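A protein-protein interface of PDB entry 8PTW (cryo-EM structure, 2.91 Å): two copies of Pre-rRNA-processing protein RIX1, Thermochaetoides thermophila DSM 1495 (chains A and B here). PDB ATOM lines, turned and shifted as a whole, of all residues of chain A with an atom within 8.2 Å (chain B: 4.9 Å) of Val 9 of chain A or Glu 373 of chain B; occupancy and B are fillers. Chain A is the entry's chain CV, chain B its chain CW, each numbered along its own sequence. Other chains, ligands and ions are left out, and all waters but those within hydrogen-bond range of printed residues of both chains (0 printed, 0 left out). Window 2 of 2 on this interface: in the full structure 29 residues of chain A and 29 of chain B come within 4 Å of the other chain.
The side-chain carboxylate (OD1) of Asp 6 of chain A sits at hydrogen-bond distance from the side-chain hydroxyl (OG) of Ser 376 of chain B (2.9 Å).
NE2 of Gln 307 of chain B sits at hydrogen-bond distance from NE2 of His 32 of chain A.
The guanidinium group (NH2) of Arg 35 of chain A lies within hydrogen-bond range of the backbone carbonyl oxygen (O) of Ser 376 of chain B (3.4 Å).
OD1 of Asp 6 of chain A is in salt-bridge range of NE of Arg 35 of chain A, at 3.3 Å.
A ring nitrogen (ND1) of His 32 of chain A lies close to the guanidinium group (NH2) of Arg 35 of chain A (3.1 Å).
The backbone carbonyl oxygen (O) of His 32 of chain A is in hydrogen-bond range of the side-chain sulfur (SG) of Cys 36 of chain A, 3.2 Å away.
The side-chain hydroxyl of Ser 376 of chain B lies within hydrogen-bond range of the backbone carbonyl oxygen of Ala 372 of chain B, 3.1 Å away.
Ala 372 of chain B touches Pro 5 of chain A (O to CB, 3.7 Å).
Pro 5 of chain A touches Ser 376 of chain B.
CA of Glu 373 of chain B touches CG2 of Val 9 of chain A, 3.9 Å away.
Ser 376 of chain B touches Val 9 of chain A (OG to CG2, 3.7 Å).
CE1 of His 32 of chain A touches CB of Ser 376 of chain B, at 3.6 Å.
Of the printed residues of chain B, Asp 6 of chain A touches Ser 376 (2.9 Å).
Val 9 of chain A touches two residues of chain B.
Ala 15 of chain A touches none of the printed residues of chain B.
Of the printed residues of chain A, Gln 307 of chain B touches His 32 (3.4 Å).
Printed residues of chain A within 4 Å of Ala 372 of chain B: Pro 5 (3.7 Å).
Of chain A, only Val 9 (3.9 Å) comes within 4 Å of Glu 373 of chain B.
Leu 374 of chain B touches none of the printed residues of chain A.
The nearest residue of chain A that does not touch Glu 373 of chain B is Arg 13 of chain A (4.4 Å).
Hydrophobic or aromatic side chains of chain B within 4 Å of the printed part of chain A: Ala 372.
Printed residues of chain A that touch a printed residue of chain B: Pro 5, Asp 6, Val 9, His 32 and Arg 35.
Hydrophobic or aromatic side chains of chain A that line the printed part of chain B: Pro 5, Val 9 and His 32.
Among the printed residues, no Asp or Glu carboxylate lies within 4 Å of a Lys or Arg side-chain nitrogen of the other chain.
No position is printed for both chains.
Of the 8 pairs that touch across the chains among the printed residues, none has its exchanged pair printed and touching as well.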
ATOM      1  N   ALA A   3       4.208   6.307  -6.091  1.00  0.00           N
ATOM      2  CA  ALA A   3       4.039   6.242  -4.652  1.00  0.00           C
ATOM      3  C   ALA A   3       4.849   7.342  -3.962  1.00  0.00           C
ATOM      4  O   ALA A   3       5.832   7.839  -4.518  1.00  0.00           O
ATOM      5  CB  ALA A   3       4.471   4.875  -4.132  1.00  0.00           C
ATOM      6  N   PRO A   4       4.442   7.754  -2.763  1.00  0.00           N
ATOM      7  CA  PRO A   4       5.289   8.637  -1.949  1.00  0.00           C
ATOM      8  C   PRO A   4       6.586   7.946  -1.570  1.00  0.00           C
ATOM      9  O   PRO A   4       6.627   6.710  -1.471  1.00  0.00           O
ATOM     10  CB  PRO A   4       4.422   8.919  -0.712  1.00  0.00           C
ATOM     11  CG  PRO A   4       3.032   8.691  -1.165  1.00  0.00           C
ATOM     12  CD  PRO A   4       3.100   7.592  -2.178  1.00  0.00           C
ATOM     13  N   PRO A   5       7.680   8.709  -1.381  1.00  0.00           N
ATOM     14  CA  PRO A   5       8.981   8.091  -1.080  1.00  0.00           C
ATOM     15  C   PRO A   5       9.013   7.298   0.217  1.00  0.00           C
ATOM     16  O   PRO A   5       9.706   6.278   0.305  1.00  0.00           O
ATOM     17  CB  PRO A   5       9.929   9.298  -1.009  1.00  0.00           C
ATOM     18  CG  PRO A   5       9.047  10.457  -0.703  1.00  0.00           C
ATOM     19  CD  PRO A   5       7.764  10.179  -1.418  1.00  0.00           C
ATOM     20  N   ASP A   6       8.259   7.759   1.220  1.00  0.00           N
ATOM     21  CA  ASP A   6       8.279   7.127   2.536  1.00  0.00           C
ATOM     22  C   ASP A   6       7.770   5.693   2.480  1.00  0.00           C
ATOM     23  O   ASP A   6       8.359   4.795   3.091  1.00  0.00           O
ATOM     24  CB  ASP A   6       7.444   7.945   3.521  1.00  0.00           C
ATOM     25  CG  ASP A   6       8.015   9.325   3.767  1.00  0.00           C
ATOM     26  OD1 ASP A   6       9.250   9.447   3.902  1.00  0.00           O
ATOM     27  OD2 ASP A   6       7.227  10.291   3.822  1.00  0.00           O
ATOM     28  N   LEU A   7       6.688   5.460   1.733  1.00  0.00           N
ATOM     29  CA  LEU A   7       6.103   4.124   1.654  1.00  0.00           C
ATOM     30  C   LEU A   7       7.027   3.152   0.927  1.00  0.00           C
ATOM     31  O   LEU A   7       7.164   1.990   1.335  1.00  0.00           O
ATOM     32  CB  LEU A   7       4.741   4.204   0.967  1.00  0.00           C
ATOM     33  CG  LEU A   7       3.992   2.907   0.665  1.00  0.00           C
ATOM     34  CD1 LEU A   7       3.748   2.116   1.938  1.00  0.00           C
ATOM     35  CD2 LEU A   7       2.682   3.232  -0.025  1.00  0.00           C
ATOM     36  N   ARG A   8       7.678   3.613  -0.144  1.00  0.00           N
ATOM     37  CA  ARG A   8       8.627   2.766  -0.863  1.00  0.00           C
ATOM     38  C   ARG A   8       9.854   2.463  -0.012  1.00  0.00           C
ATOM     39  O   ARG A   8      10.386   1.345  -0.054  1.00  0.00           O
ATOM     40  CB  ARG A   8       9.033   3.436  -2.174  1.00  0.00           C
ATOM     41  CG  ARG A   8       9.912   2.584  -3.069  1.00  0.00           C
ATOM     42  CD  ARG A   8      10.195   3.293  -4.382  1.00  0.00           C
ATOM     43  NE  ARG A   8       8.983   3.466  -5.175  1.00  0.00           N
ATOM     44  CZ  ARG A   8       8.404   4.636  -5.413  1.00  0.00           C
ATOM     45  NH1 ARG A   8       8.895   5.763  -4.925  1.00  0.00           N
ATOM     46  NH2 ARG A   8       7.304   4.674  -6.160  1.00  0.00           N
ATOM     47  N   VAL A   9      10.313   3.445   0.770  1.00  0.00           N
ATOM     48  CA  VAL A   9      11.413   3.211   1.704  1.00  0.00           C
ATOM     49  C   VAL A   9      11.017   2.172   2.748  1.00  0.00           C
ATOM     50  O   VAL A   9      11.803   1.272   3.073  1.00  0.00           O
ATOM     51  CB  VAL A   9      11.861   4.539   2.346  1.00  0.00           C
ATOM     52  CG1 VAL A   9      12.727   4.295   3.566  1.00  0.00           C
ATOM     53  CG2 VAL A   9      12.638   5.367   1.340  1.00  0.00           C
ATOM     54  N   VAL A  10       9.785   2.263   3.265  1.00  0.00           N
ATOM     55  CA  VAL A  10       9.287   1.276   4.223  1.00  0.00           C
ATOM     56  C   VAL A  10       9.280  -0.118   3.612  1.00  0.00           C
ATOM     57  O   VAL A  10       9.750  -1.081   4.231  1.00  0.00           O
ATOM     58  CB  VAL A  10       7.881   1.664   4.720  1.00  0.00           C
ATOM     59  CG1 VAL A  10       7.270   0.532   5.500  1.00  0.00           C
ATOM     60  CG2 VAL A  10       7.955   2.853   5.610  1.00  0.00           C
ATOM     61  N   CYS A  11       8.765  -0.241   2.386  1.00  0.00           N
ATOM     62  CA  CYS A  11       8.692  -1.548   1.736  1.00  0.00           C
ATOM     63  C   CYS A  11      10.080  -2.130   1.487  1.00  0.00           C
ATOM     64  O   CYS A  11      10.317  -3.318   1.744  1.00  0.00           O
ATOM     65  CB  CYS A  11       7.910  -1.441   0.428  1.00  0.00           C
ATOM     66  SG  CYS A  11       6.150  -1.112   0.644  1.00  0.00           S
ATOM     67  N   HIS A  12      11.020  -1.302   1.020  1.00  0.00           N
ATOM     68  CA  HIS A  12      12.363  -1.796   0.728  1.00  0.00           C
ATOM     69  C   HIS A  12      13.103  -2.192   2.001  1.00  0.00           C
ATOM     70  O   HIS A  12      13.791  -3.220   2.034  1.00  0.00           O
ATOM     71  CB  HIS A  12      13.153  -0.743  -0.048  1.00  0.00           C
ATOM     72  CG  HIS A  12      14.304  -1.304  -0.821  1.00  0.00           C
ATOM     73  ND1 HIS A  12      14.153  -2.299  -1.761  1.00  0.00           N
ATOM     74  CD2 HIS A  12      15.626  -1.011  -0.792  1.00  0.00           C
ATOM     75  CE1 HIS A  12      15.331  -2.595  -2.280  1.00  0.00           C
ATOM     76  NE2 HIS A  12      16.242  -1.828  -1.709  1.00  0.00           N
ATOM     77  N   ARG A  13      12.968  -1.394   3.066  1.00  0.00           N
ATOM     78  CA  ARG A  13      13.649  -1.718   4.314  1.00  0.00           C
ATOM     79  C   ARG A  13      13.024  -2.932   4.991  1.00  0.00           C
ATOM     80  O   ARG A  13      13.719  -3.698   5.663  1.00  0.00           O
ATOM     81  CB  ARG A  13      13.642  -0.511   5.255  1.00  0.00           C
ATOM     82  CG  ARG A  13      14.460   0.668   4.749  1.00  0.00           C
ATOM     83  CD  ARG A  13      15.947   0.481   4.996  1.00  0.00           C
ATOM     84  NE  ARG A  13      16.366   1.035   6.277  1.00  0.00           N
ATOM     85  CZ  ARG A  13      17.627   1.133   6.672  1.00  0.00           C
ATOM     86  NH1 ARG A  13      18.624   0.708   5.913  1.00  0.00           N
ATOM     87  NH2 ARG A  13      17.897   1.672   7.858  1.00  0.00           N
ATOM     88  N   LEU A  14      11.713  -3.126   4.828  1.00  0.00           N
ATOM     89  CA  LEU A  14      11.085  -4.319   5.381  1.00  0.00           C
ATOM     90  C   LEU A  14      11.467  -5.563   4.590  1.00  0.00           C
ATOM     91  O   LEU A  14      11.573  -6.658   5.155  1.00  0.00           O
ATOM     92  CB  LEU A  14       9.568  -4.152   5.421  1.00  0.00           C
ATOM     93  CG  LEU A  14       9.018  -3.356   6.604  1.00  0.00           C
ATOM     94  CD1 LEU A  14       7.506  -3.402   6.606  1.00  0.00           C
ATOM     95  CD2 LEU A  14       9.569  -3.887   7.914  1.00  0.00           C
ATOM     96  N   ALA A  15      11.673  -5.418   3.280  1.00  0.00           N
ATOM     97  CA  ALA A  15      12.067  -6.571   2.477  1.00  0.00           C
ATOM     98  C   ALA A  15      13.526  -6.947   2.707  1.00  0.00           C
ATOM     99  O   ALA A  15      13.866  -8.136   2.749  1.00  0.00           O
ATOM    100  CB  ALA A  15      11.810  -6.292   0.997  1.00  0.00           C
ATOM    101  N   SER A  16      14.407  -5.954   2.858  1.00  0.00           N
ATOM    102  CA  SER A  16      15.840  -6.241   2.867  1.00  0.00           C
ATOM    103  C   SER A  16      16.338  -6.669   4.245  1.00  0.00           C
ATOM    104  O   SER A  16      17.241  -7.508   4.346  1.00  0.00           O
ATOM    105  CB  SER A  16      16.618  -5.021   2.377  1.00  0.00           C
ATOM    106  OG  SER A  16      16.316  -3.877   3.153  1.00  0.00           O
ATOM    107  N   THR A  17      15.778  -6.104   5.309  1.00  0.00           N
ATOM    108  CA  THR A  17      16.352  -6.275   6.646  1.00  0.00           C
ATOM    109  C   THR A  17      16.122  -7.689   7.170  1.00  0.00           C
ATOM    110  O   THR A  17      15.035  -8.247   6.977  1.00  0.00           O
ATOM    111  CB  THR A  17      15.746  -5.260   7.616  1.00  0.00           C
ATOM    112  OG1 THR A  17      15.635  -3.986   6.969  1.00  0.00           O
ATOM    113  CG2 THR A  17      16.611  -5.106   8.850  1.00  0.00           C
ATOM    114  N   LEU A  28      13.166   4.293  13.011  1.00  0.00           N
ATOM    115  CA  LEU A  28      13.077   4.887  11.680  1.00  0.00           C
ATOM    116  C   LEU A  28      11.884   4.333  10.907  1.00  0.00           C
ATOM    117  O   LEU A  28      11.236   5.063  10.148  1.00  0.00           O
ATOM    118  CB  LEU A  28      14.392   4.681  10.919  1.00  0.00           C
ATOM    119  CG  LEU A  28      14.979   3.307  10.567  1.00  0.00           C
ATOM    120  CD1 LEU A  28      14.419   2.720   9.269  1.00  0.00           C
ATOM    121  CD2 LEU A  28      16.497   3.381  10.512  1.00  0.00           C
ATOM    122  N   LEU A  29      11.572   3.047  11.100  1.00  0.00           N
ATOM    123  CA  LEU A  29      10.393   2.465  10.467  1.00  0.00           C
ATOM    124  C   LEU A  29       9.115   3.113  10.982  1.00  0.00           C
ATOM    125  O   LEU A  29       8.207   3.415  10.198  1.00  0.00           O
ATOM    126  CB  LEU A  29      10.354   0.955  10.699  1.00  0.00           C
ATOM    127  CG  LEU A  29      11.420   0.112   9.999  1.00  0.00           C
ATOM    128  CD1 LEU A  29      11.506  -1.267  10.632  1.00  0.00           C
ATOM    129  CD2 LEU A  29      11.125   0.005   8.513  1.00  0.00           C
ATOM    130  N   HIS A  32       8.869   6.637   9.465  1.00  0.00           N
ATOM    131  CA  HIS A  32       8.462   6.606   8.066  1.00  0.00           C
ATOM    132  C   HIS A  32       6.998   6.206   7.903  1.00  0.00           C
ATOM    133  O   HIS A  32       6.313   6.714   7.010  1.00  0.00           O
ATOM    134  CB  HIS A  32       9.363   5.661   7.275  1.00  0.00           C
ATOM    135  CG  HIS A  32      10.769   6.144   7.117  1.00  0.00           C
ATOM    136  ND1 HIS A  32      11.074   7.427   6.718  1.00  0.00           N
ATOM    137  CD2 HIS A  32      11.953   5.524   7.331  1.00  0.00           C
ATOM    138  CE1 HIS A  32      12.387   7.571   6.677  1.00  0.00           C
ATOM    139  NE2 HIS A  32      12.943   6.431   7.044  1.00  0.00           N
ATOM    140  N   VAL A  33       6.493   5.297   8.744  1.00  0.00           N
ATOM    141  CA  VAL A  33       5.098   4.883   8.585  1.00  0.00           C
ATOM    142  C   VAL A  33       4.157   5.916   9.203  1.00  0.00           C
ATOM    143  O   VAL A  33       3.005   6.063   8.774  1.00  0.00           O
ATOM    144  CB  VAL A  33       4.876   3.465   9.155  1.00  0.00           C
ATOM    145  CG1 VAL A  33       5.020   3.437  10.642  1.00  0.00           C
ATOM    146  CG2 VAL A  33       3.514   2.933   8.759  1.00  0.00           C
ATOM    147  N   ARG A  35       4.840   8.964   8.754  1.00  0.00           N
ATOM    148  CA  ARG A  35       4.845   9.955   7.682  1.00  0.00           C
ATOM    149  C   ARG A  35       3.770   9.659   6.635  1.00  0.00           C
ATOM    150  O   ARG A  35       3.071  10.572   6.182  1.00  0.00           O
ATOM    151  CB  ARG A  35       6.228  10.013   7.034  1.00  0.00           C
ATOM    152  CG  ARG A  35       7.176  11.013   7.684  1.00  0.00           C
ATOM    153  CD  ARG A  35       8.307  11.415   6.746  1.00  0.00           C
ATOM    154  NE  ARG A  35       9.535  10.662   6.979  1.00  0.00           N
ATOM    155  CZ  ARG A  35      10.404  10.908   7.951  1.00  0.00           C
ATOM    156  NH1 ARG A  35      10.203  11.872   8.832  1.00  0.00           N
ATOM    157  NH2 ARG A  35      11.503  10.166   8.042  1.00  0.00           N
ATOM    158  N   CYS A  36       3.620   8.393   6.242  1.00  0.00           N
ATOM    159  CA  CYS A  36       2.710   8.022   5.155  1.00  0.00           C
ATOM    160  C   CYS A  36       1.366   7.518   5.691  1.00  0.00           C
ATOM    161  O   CYS A  36       0.950   6.385   5.454  1.00  0.00           O
ATOM    162  CB  CYS A  36       3.362   6.985   4.246  1.00  0.00           C
ATOM    163  SG  CYS A  36       4.024   5.519   5.077  1.00  0.00           S
ATOM    164  N   LEU A  58       1.647  -0.972  -2.974  1.00  0.00           N
ATOM    165  CA  LEU A  58       2.638  -0.944  -1.903  1.00  0.00           C
ATOM    166  C   LEU A  58       1.976  -0.982  -0.531  1.00  0.00           C
ATOM    167  O   LEU A  58       2.520  -1.577   0.405  1.00  0.00           O
ATOM    168  CB  LEU A  58       3.534   0.284  -2.040  1.00  0.00           C
ATOM    169  CG  LEU A  58       4.585   0.221  -3.148  1.00  0.00           C
ATOM    170  CD1 LEU A  58       5.459   1.459  -3.115  1.00  0.00           C
ATOM    171  CD2 LEU A  58       5.427  -1.037  -3.020  1.00  0.00           C
ATOM    172  N   LEU B 306      22.766   5.610   3.065  1.00  0.00           N
ATOM    173  CA  LEU B 306      22.308   6.995   3.096  1.00  0.00           C
ATOM    174  C   LEU B 306      21.598   7.320   4.403  1.00  0.00           C
ATOM    175  O   LEU B 306      21.731   8.431   4.929  1.00  0.00           O
ATOM    176  CB  LEU B 306      21.392   7.266   1.906  1.00  0.00           C
ATOM    177  CG  LEU B 306      21.036   8.729   1.665  1.00  0.00           C
ATOM    178  CD1 LEU B 306      22.292   9.568   1.549  1.00  0.00           C
ATOM    179  CD2 LEU B 306      20.218   8.839   0.409  1.00  0.00           C
ATOM    180  N   GLN B 307      20.833   6.364   4.937  1.00  0.00           N
ATOM    181  CA  GLN B 307      20.174   6.581   6.221  1.00  0.00           C
ATOM    182  C   GLN B 307      21.189   6.676   7.353  1.00  0.00           C
ATOM    183  O   GLN B 307      21.037   7.497   8.265  1.00  0.00           O
ATOM    184  CB  GLN B 307      19.167   5.464   6.491  1.00  0.00           C
ATOM    185  CG  GLN B 307      18.284   5.713   7.702  1.00  0.00           C
ATOM    186  CD  GLN B 307      17.410   6.941   7.538  1.00  0.00           C
ATOM    187  OE1 GLN B 307      17.678   7.991   8.123  1.00  0.00           O
ATOM    188  NE2 GLN B 307      16.356   6.814   6.741  1.00  0.00           N
ATOM    189  N   ASP B 369      15.899   4.833  -5.920  1.00  0.00           N
ATOM    190  CA  ASP B 369      15.703   4.447  -4.524  1.00  0.00           C
ATOM    191  C   ASP B 369      16.540   5.307  -3.584  1.00  0.00           C
ATOM    192  O   ASP B 369      16.080   5.678  -2.496  1.00  0.00           O
ATOM    193  CB  ASP B 369      16.036   2.968  -4.339  1.00  0.00           C
ATOM    194  CG  ASP B 369      15.075   2.058  -5.077  1.00  0.00           C
ATOM    195  OD1 ASP B 369      14.228   2.576  -5.835  1.00  0.00           O
ATOM    196  OD2 ASP B 369      15.165   0.826  -4.901  1.00  0.00           O
ATOM    197  N   GLU B 370      17.773   5.632  -3.986  1.00  0.00           N
ATOM    198  CA  GLU B 370      18.605   6.518  -3.177  1.00  0.00           C
ATOM    199  C   GLU B 370      18.007   7.918  -3.111  1.00  0.00           C
ATOM    200  O   GLU B 370      18.053   8.571  -2.063  1.00  0.00           O
ATOM    201  CB  GLU B 370      20.028   6.557  -3.735  1.00  0.00           C
ATOM    202  CG  GLU B 370      20.932   7.587  -3.077  1.00  0.00           C
ATOM    203  CD  GLU B 370      22.389   7.404  -3.437  1.00  0.00           C
ATOM    204  OE1 GLU B 370      22.713   6.428  -4.145  1.00  0.00           O
ATOM    205  OE2 GLU B 370      23.213   8.239  -3.010  1.00  0.00           O
ATOM    206  N   LYS B 371      17.418   8.382  -4.216  1.00  0.00           N
ATOM    207  CA  LYS B 371      16.727   9.667  -4.209  1.00  0.00           C
ATOM    208  C   LYS B 371      15.544   9.655  -3.250  1.00  0.00           C
ATOM    209  O   LYS B 371      15.335  10.619  -2.502  1.00  0.00           O
ATOM    210  CB  LYS B 371      16.265  10.023  -5.622  1.00  0.00           C
ATOM    211  CG  LYS B 371      17.391  10.191  -6.624  1.00  0.00           C
ATOM    212  CD  LYS B 371      16.853  10.305  -8.039  1.00  0.00           C
ATOM    213  CE  LYS B 371      17.968  10.575  -9.033  1.00  0.00           C
ATOM    214  NZ  LYS B 371      17.452  10.681 -10.425  1.00  0.00           N
ATOM    215  N   ALA B 372      14.768   8.565  -3.248  1.00  0.00           N
ATOM    216  CA  ALA B 372      13.626   8.457  -2.344  1.00  0.00           C
ATOM    217  C   ALA B 372      14.074   8.428  -0.886  1.00  0.00           C
ATOM    218  O   ALA B 372      13.460   9.065  -0.019  1.00  0.00           O
ATOM    219  CB  ALA B 372      12.810   7.210  -2.682  1.00  0.00           C
ATOM    220  N   GLU B 373      15.160   7.701  -0.603  1.00  0.00           N
ATOM    221  CA  GLU B 373      15.699   7.661   0.754  1.00  0.00           C
ATOM    222  C   GLU B 373      16.215   9.031   1.186  1.00  0.00           C
ATOM    223  O   GLU B 373      16.066   9.418   2.350  1.00  0.00           O
ATOM    224  CB  GLU B 373      16.807   6.614   0.849  1.00  0.00           C
ATOM    225  CG  GLU B 373      17.093   6.144   2.263  1.00  0.00           C
ATOM    226  CD  GLU B 373      18.066   4.983   2.305  1.00  0.00           C
ATOM    227  OE1 GLU B 373      18.855   4.834   1.349  1.00  0.00           O
ATOM    228  OE2 GLU B 373      18.042   4.218   3.292  1.00  0.00           O
ATOM    229  N   LEU B 374      16.817   9.780   0.259  1.00  0.00           N
ATOM    230  CA  LEU B 374      17.269  11.132   0.570  1.00  0.00           C
ATOM    231  C   LEU B 374      16.098  12.057   0.873  1.00  0.00           C
ATOM    232  O   LEU B 374      16.157  12.858   1.817  1.00  0.00           O
ATOM    233  CB  LEU B 374      18.100  11.681  -0.589  1.00  0.00           C
ATOM    234  CG  LEU B 374      18.557  13.135  -0.505  1.00  0.00           C
ATOM    235  CD1 LEU B 374      19.415  13.360   0.725  1.00  0.00           C
ATOM    236  CD2 LEU B 374      19.324  13.495  -1.756  1.00  0.00           C
ATOM    237  N   TRP B 375      15.024  11.963   0.079  1.00  0.00           N
ATOM    238  CA  TRP B 375      13.847  12.791   0.330  1.00  0.00           C
ATOM    239  C   TRP B 375      13.197  12.428   1.658  1.00  0.00           C
ATOM    240  O   TRP B 375      12.607  13.286   2.325  1.00  0.00           O
ATOM    241  CB  TRP B 375      12.827  12.659  -0.806  1.00  0.00           C
ATOM    242  CG  TRP B 375      13.306  12.887  -2.242  1.00  0.00           C
ATOM    243  CD1 TRP B 375      12.889  12.191  -3.340  1.00  0.00           C
ATOM    244  CD2 TRP B 375      14.234  13.880  -2.734  1.00  0.00           C
ATOM    245  NE1 TRP B 375      13.507  12.660  -4.470  1.00  0.00           N
ATOM    246  CE2 TRP B 375      14.332  13.699  -4.129  1.00  0.00           C
ATOM    247  CE3 TRP B 375      14.988  14.899  -2.137  1.00  0.00           C
ATOM    248  CZ2 TRP B 375      15.155  14.487  -4.928  1.00  0.00           C
ATOM    249  CZ3 TRP B 375      15.805  15.676  -2.934  1.00  0.00           C
ATOM    250  CH2 TRP B 375      15.881  15.467  -4.314  1.00  0.00           C
ATOM    251  N   SER B 376      13.293  11.157   2.056  1.00  0.00           N
ATOM    252  CA  SER B 376      12.799  10.759   3.370  1.00  0.00           C
ATOM    253  C   SER B 376      13.698  11.279   4.488  1.00  0.00           C
ATOM    254  O   SER B 376      13.212  11.642   5.565  1.00  0.00           O
ATOM    255  CB  SER B 376      12.683   9.238   3.444  1.00  0.00           C
ATOM    256  OG  SER B 376      11.722   8.754   2.524  1.00  0.00           O
ATOM    257  N   ALA B 377      15.013  11.316   4.253  1.00  0.00           N
ATOM    258  CA  ALA B 377      15.954  11.579   5.339  1.00  0.00           C
ATOM    259  C   ALA B 377      16.174  13.071   5.570  1.00  0.00           C
ATOM    260  O   ALA B 377      16.666  13.468   6.632  1.00  0.00           O
ATOM    261  CB  ALA B 377      17.283  10.884   5.055  1.00  0.00           C
